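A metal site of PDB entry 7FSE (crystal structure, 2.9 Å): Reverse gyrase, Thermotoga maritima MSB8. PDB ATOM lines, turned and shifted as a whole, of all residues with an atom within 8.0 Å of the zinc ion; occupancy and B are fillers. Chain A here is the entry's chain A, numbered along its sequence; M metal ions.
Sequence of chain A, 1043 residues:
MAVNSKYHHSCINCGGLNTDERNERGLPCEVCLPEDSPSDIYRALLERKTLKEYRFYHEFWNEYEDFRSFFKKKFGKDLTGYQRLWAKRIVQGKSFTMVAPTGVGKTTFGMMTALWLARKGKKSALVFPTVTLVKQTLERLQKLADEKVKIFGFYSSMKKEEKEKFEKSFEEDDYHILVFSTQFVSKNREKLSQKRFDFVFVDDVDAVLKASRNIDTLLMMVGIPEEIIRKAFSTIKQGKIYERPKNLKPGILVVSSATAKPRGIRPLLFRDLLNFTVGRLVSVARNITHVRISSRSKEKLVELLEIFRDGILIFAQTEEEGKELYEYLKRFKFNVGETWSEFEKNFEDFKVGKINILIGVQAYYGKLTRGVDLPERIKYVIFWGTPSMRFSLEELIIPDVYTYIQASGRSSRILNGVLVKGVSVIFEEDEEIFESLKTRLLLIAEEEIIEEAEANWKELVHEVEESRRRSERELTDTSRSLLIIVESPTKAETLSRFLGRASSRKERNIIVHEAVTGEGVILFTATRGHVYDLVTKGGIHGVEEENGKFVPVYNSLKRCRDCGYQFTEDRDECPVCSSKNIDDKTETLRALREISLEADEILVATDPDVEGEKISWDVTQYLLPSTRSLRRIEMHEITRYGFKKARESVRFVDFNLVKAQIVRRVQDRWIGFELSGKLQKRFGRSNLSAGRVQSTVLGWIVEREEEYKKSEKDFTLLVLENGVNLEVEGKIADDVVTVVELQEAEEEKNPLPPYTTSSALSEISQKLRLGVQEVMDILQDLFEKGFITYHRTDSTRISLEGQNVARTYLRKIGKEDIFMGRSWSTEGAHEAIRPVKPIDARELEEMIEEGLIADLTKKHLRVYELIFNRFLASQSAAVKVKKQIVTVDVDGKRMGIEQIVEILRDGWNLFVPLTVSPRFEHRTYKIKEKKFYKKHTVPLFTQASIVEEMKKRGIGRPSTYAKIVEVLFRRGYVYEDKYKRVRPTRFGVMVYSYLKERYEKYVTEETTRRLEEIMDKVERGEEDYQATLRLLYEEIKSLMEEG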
ATOM      1  N   SER A  10      -5.542 -13.871  -6.269  1.00  0.00           N
ATOM      2  CA  SER A  10      -5.804 -13.395  -7.614  1.00  0.00           C
ATOM      3  C   SER A  10      -4.545 -13.184  -8.450  1.00  0.00           C
ATOM      4  O   SER A  10      -4.657 -13.032  -9.669  1.00  0.00           O
ATOM      5  CB  SER A  10      -6.600 -12.090  -7.570  1.00  0.00           C
ATOM      6  OG  SER A  10      -5.887 -11.079  -6.885  1.00  0.00           O
ATOM      7  N   CYS A  11      -3.363 -13.160  -7.843  1.00  0.00           N
ATOM      8  CA  CYS A  11      -2.141 -12.985  -8.627  1.00  0.00           C
ATOM      9  C   CYS A  11      -1.933 -14.180  -9.533  1.00  0.00           C
ATOM     10  O   CYS A  11      -1.949 -15.331  -9.080  1.00  0.00           O
ATOM     11  CB  CYS A  11      -0.933 -12.789  -7.708  1.00  0.00           C
ATOM     12  SG  CYS A  11       0.603 -12.463  -8.626  1.00  0.00           S
ATOM     13  N   ILE A  12      -1.727 -13.909 -10.820  1.00  0.00           N
ATOM     14  CA  ILE A  12      -1.630 -14.984 -11.795  1.00  0.00           C
ATOM     15  C   ILE A  12      -0.248 -15.640 -11.793  1.00  0.00           C
ATOM     16  O   ILE A  12      -0.105 -16.766 -12.272  1.00  0.00           O
ATOM     17  CB  ILE A  12      -1.983 -14.458 -13.195  1.00  0.00           C
ATOM     18  CG1 ILE A  12      -2.246 -15.612 -14.161  1.00  0.00           C
ATOM     19  CG2 ILE A  12      -0.899 -13.530 -13.706  1.00  0.00           C
ATOM     20  CD1 ILE A  12      -2.764 -15.178 -15.507  1.00  0.00           C
ATOM     21  N   ASN A  13       0.766 -14.982 -11.230  1.00  0.00           N
ATOM     22  CA  ASN A  13       2.125 -15.504 -11.240  1.00  0.00           C
ATOM     23  C   ASN A  13       2.542 -16.150  -9.928  1.00  0.00           C
ATOM     24  O   ASN A  13       3.159 -17.222  -9.944  1.00  0.00           O
ATOM     25  CB  ASN A  13       3.122 -14.395 -11.586  1.00  0.00           C
ATOM     26  CG  ASN A  13       4.553 -14.875 -11.540  1.00  0.00           C
ATOM     27  OD1 ASN A  13       5.012 -15.589 -12.427  1.00  0.00           O
ATOM     28  ND2 ASN A  13       5.277 -14.501 -10.485  1.00  0.00           N
ATOM     29  N   CYS A  14       2.241 -15.536  -8.793  1.00  0.00           N
ATOM     30  CA  CYS A  14       2.625 -16.106  -7.505  1.00  0.00           C
ATOM     31  C   CYS A  14       1.446 -16.722  -6.753  1.00  0.00           C
ATOM     32  O   CYS A  14       1.668 -17.368  -5.722  1.00  0.00           O
ATOM     33  CB  CYS A  14       3.306 -15.054  -6.624  1.00  0.00           C
ATOM     34  SG  CYS A  14       2.189 -13.956  -5.719  1.00  0.00           S
ATOM     35  N   GLY A  15       0.219 -16.541  -7.240  1.00  0.00           N
ATOM     36  CA  GLY A  15      -0.929 -17.103  -6.568  1.00  0.00           C
ATOM     37  C   GLY A  15      -1.291 -16.438  -5.264  1.00  0.00           C
ATOM     38  O   GLY A  15      -2.159 -16.943  -4.538  1.00  0.00           O
ATOM     39  N   GLY A  16      -0.664 -15.308  -4.937  1.00  0.00           N
ATOM     40  CA  GLY A  16      -0.872 -14.612  -3.692  1.00  0.00           C
ATOM     41  C   GLY A  16      -1.833 -13.443  -3.822  1.00  0.00           C
ATOM     42  O   GLY A  16      -2.721 -13.441  -4.678  1.00  0.00           O
ATOM     43  N   LEU A  17      -1.650 -12.455  -2.964  1.00  0.00           N
ATOM     44  CA  LEU A  17      -2.557 -11.314  -2.881  1.00  0.00           C
ATOM     45  C   LEU A  17      -2.167 -10.256  -3.904  1.00  0.00           C
ATOM     46  O   LEU A  17      -0.983  -9.898  -4.018  1.00  0.00           O
ATOM     47  CB  LEU A  17      -2.536 -10.726  -1.468  1.00  0.00           C
ATOM     48  CG  LEU A  17      -3.414  -9.513  -1.167  1.00  0.00           C
ATOM     49  CD1 LEU A  17      -4.128  -9.689   0.164  1.00  0.00           C
ATOM     50  CD2 LEU A  17      -2.588  -8.236  -1.164  1.00  0.00           C
ATOM     51  N   ASN A  18      -3.158  -9.747  -4.634  1.00  0.00           N
ATOM     52  CA  ASN A  18      -2.965  -8.675  -5.596  1.00  0.00           C
ATOM     53  C   ASN A  18      -4.138  -7.713  -5.491  1.00  0.00           C
ATOM     54  O   ASN A  18      -5.242  -8.082  -5.074  1.00  0.00           O
ATOM     55  CB  ASN A  18      -2.833  -9.206  -7.029  1.00  0.00           C
ATOM     56  CG  ASN A  18      -2.486  -8.126  -8.027  1.00  0.00           C
ATOM     57  OD1 ASN A  18      -2.036  -7.040  -7.657  1.00  0.00           O
ATOM     58  ND2 ASN A  18      -2.668  -8.419  -9.312  1.00  0.00           N
ATOM     59  N   LEU A  27      -2.083  -7.390 -14.737  1.00  0.00           N
ATOM     60  CA  LEU A  27      -0.724  -7.528 -14.247  1.00  0.00           C
ATOM     61  C   LEU A  27      -0.685  -8.308 -12.928  1.00  0.00           C
ATOM     62  O   LEU A  27      -1.668  -8.346 -12.187  1.00  0.00           O
ATOM     63  CB  LEU A  27      -0.062  -6.157 -14.019  1.00  0.00           C
ATOM     64  CG  LEU A  27       0.492  -5.434 -15.241  1.00  0.00           C
ATOM     65  CD1 LEU A  27      -0.593  -4.671 -15.991  1.00  0.00           C
ATOM     66  CD2 LEU A  27       1.634  -4.517 -14.836  1.00  0.00           C
ATOM     67  N   PRO A  28       0.454  -8.950 -12.629  1.00  0.00           N
ATOM     68  CA  PRO A  28       0.616  -9.584 -11.309  1.00  0.00           C
ATOM     69  C   PRO A  28       0.733  -8.567 -10.190  1.00  0.00           C
ATOM     70  O   PRO A  28       0.620  -7.359 -10.418  1.00  0.00           O
ATOM     71  CB  PRO A  28       1.905 -10.401 -11.465  1.00  0.00           C
ATOM     72  CG  PRO A  28       2.073 -10.570 -12.949  1.00  0.00           C
ATOM     73  CD  PRO A  28       1.543  -9.304 -13.547  1.00  0.00           C
ATOM     74  N   CYS A  29       0.965  -9.038  -8.970  1.00  0.00           N
ATOM     75  CA  CYS A  29       0.997  -8.162  -7.814  1.00  0.00           C
ATOM     76  C   CYS A  29       2.275  -7.319  -7.796  1.00  0.00           C
ATOM     77  O   CYS A  29       3.198  -7.520  -8.586  1.00  0.00           O
ATOM     78  CB  CYS A  29       0.861  -8.960  -6.519  1.00  0.00           C
ATOM     79  SG  CYS A  29       2.241 -10.079  -6.170  1.00  0.00           S
ATOM     80  N   GLU A  30       2.321  -6.369  -6.855  1.00  0.00           N
ATOM     81  CA  GLU A  30       3.478  -5.502  -6.737  1.00  0.00           C
ATOM     82  C   GLU A  30       4.735  -6.289  -6.395  1.00  0.00           C
ATOM     83  O   GLU A  30       5.839  -5.940  -6.835  1.00  0.00           O
ATOM     84  CB  GLU A  30       3.219  -4.435  -5.670  1.00  0.00           C
ATOM     85  CG  GLU A  30       3.784  -3.059  -6.004  1.00  0.00           C
ATOM     86  CD  GLU A  30       2.767  -2.153  -6.686  1.00  0.00           C
ATOM     87  OE1 GLU A  30       1.712  -1.882  -6.071  1.00  0.00           O
ATOM     88  OE2 GLU A  30       3.008  -1.739  -7.831  1.00  0.00           O
ATOM     89  N   VAL A  31       4.600  -7.360  -5.606  1.00  0.00           N
ATOM     90  CA  VAL A  31       5.750  -8.151  -5.200  1.00  0.00           C
ATOM     91  C   VAL A  31       6.411  -8.812  -6.407  1.00  0.00           C
ATOM     92  O   VAL A  31       7.637  -8.819  -6.545  1.00  0.00           O
ATOM     93  CB  VAL A  31       5.334  -9.201  -4.144  1.00  0.00           C
ATOM     94  CG1 VAL A  31       6.539 -10.006  -3.684  1.00  0.00           C
ATOM     95  CG2 VAL A  31       4.653  -8.519  -2.968  1.00  0.00           C
ATOM     96  N   CYS A  32       5.596  -9.372  -7.309  1.00  0.00           N
ATOM     97  CA  CYS A  32       6.155 -10.069  -8.470  1.00  0.00           C
ATOM     98  C   CYS A  32       6.798  -9.096  -9.448  1.00  0.00           C
ATOM     99  O   CYS A  32       7.920  -9.319  -9.921  1.00  0.00           O
ATOM    100  CB  CYS A  32       5.065 -10.884  -9.158  1.00  0.00           C
ATOM    101  SG  CYS A  32       4.477 -12.313  -8.218  1.00  0.00           S
ATOM    102  N   LEU A  33       6.101  -8.003  -9.764  1.00  0.00           N
ATOM    103  CA  LEU A  33       6.562  -7.073 -10.795  1.00  0.00           C
ATOM    104  C   LEU A  33       6.089  -5.673 -10.426  1.00  0.00           C
ATOM    105  O   LEU A  33       4.926  -5.311 -10.647  1.00  0.00           O
ATOM    106  CB  LEU A  33       6.038  -7.478 -12.170  1.00  0.00           C
ATOM    107  CG  LEU A  33       6.383  -6.536 -13.322  1.00  0.00           C
ATOM    108  CD1 LEU A  33       7.879  -6.286 -13.376  1.00  0.00           C
ATOM    109  CD2 LEU A  33       5.869  -7.093 -14.628  1.00  0.00           C
ATOM    110  N   LEU A  45       9.214 -10.603 -15.444  1.00  0.00           N
ATOM    111  CA  LEU A  45       9.260 -11.581 -14.360  1.00  0.00           C
ATOM    112  C   LEU A  45      10.522 -12.435 -14.437  1.00  0.00           C
ATOM    113  O   LEU A  45      11.102 -12.776 -13.402  1.00  0.00           O
ATOM    114  CB  LEU A  45       8.007 -12.453 -14.388  1.00  0.00           C
ATOM    115  CG  LEU A  45       6.724 -11.784 -13.912  1.00  0.00           C
ATOM    116  CD1 LEU A  45       5.502 -12.548 -14.405  1.00  0.00           C
ATOM    117  CD2 LEU A  45       6.714 -11.709 -12.391  1.00  0.00           C
ATOM    118  N   THR A  50      11.464 -13.777 -10.500  1.00  0.00           N
ATOM    119  CA  THR A  50      10.239 -14.048  -9.761  1.00  0.00           C
ATOM    120  C   THR A  50       9.256 -14.875 -10.582  1.00  0.00           C
ATOM    121  O   THR A  50       8.079 -14.977 -10.207  1.00  0.00           O
ATOM    122  CB  THR A  50       9.581 -12.748  -9.324  1.00  0.00           C
ATOM    123  OG1 THR A  50       9.403 -11.893 -10.458  1.00  0.00           O
ATOM    124  CG2 THR A  50      10.442 -12.031  -8.292  1.00  0.00           C
ATOM    125  N   LYS A  52       7.252 -17.733 -11.557  1.00  0.00           N
ATOM    126  CA  LYS A  52       6.826 -18.998 -10.964  1.00  0.00           C
ATOM    127  C   LYS A  52       5.719 -19.685 -11.749  1.00  0.00           C
ATOM    128  O   LYS A  52       5.906 -20.825 -12.200  1.00  0.00           O
ATOM    129  CB  LYS A  52       6.393 -18.758  -9.512  1.00  0.00           C
ATOM    130  CG  LYS A  52       7.439 -18.015  -8.687  1.00  0.00           C
ATOM    131  CD  LYS A  52       6.808 -17.353  -7.485  1.00  0.00           C
ATOM    132  CE  LYS A  52       7.734 -16.304  -6.896  1.00  0.00           C
ATOM    133  NZ  LYS A  52       7.056 -15.472  -5.869  1.00  0.00           N
HETATM  134 ZN    ZN M   1       2.401 -12.174  -7.189  1.00  0.00          ZN
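The side-chain sulfur of Cys 11 sits close to the backbone NH of Asn 13 (3.6 Å).
N of Cys 11 sits at hydrogen-bond distance from O of Gly 16 (3.2 Å).
SG of Cys 14 sits close to N of Gly 16, 3.3 Å away.
The side-chain sulfur (SG) of Cys 32 lies close to the side-chain amide nitrogen (ND2) of Asn 13 (3.3 Å).
The backbone carbonyl oxygen of Cys 32 lies within hydrogen-bond range of the side-chain hydroxyl of Thr 50 (3.0 Å).
SG of Cys 29 lies close to N of Val 31, at 3.6 Å.
Of the 19 residues printed, 4 come within 4 Å of the zinc ion.
The zinc ion is bound by SG of Cys 11 (2.3 Å), SG of Cys 14 (2.3 Å), SG of Cys 32 (2.3 Å) and SG of Cys 29 (2.3 Å).
The zinc ion has four donor atoms within binding distance.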
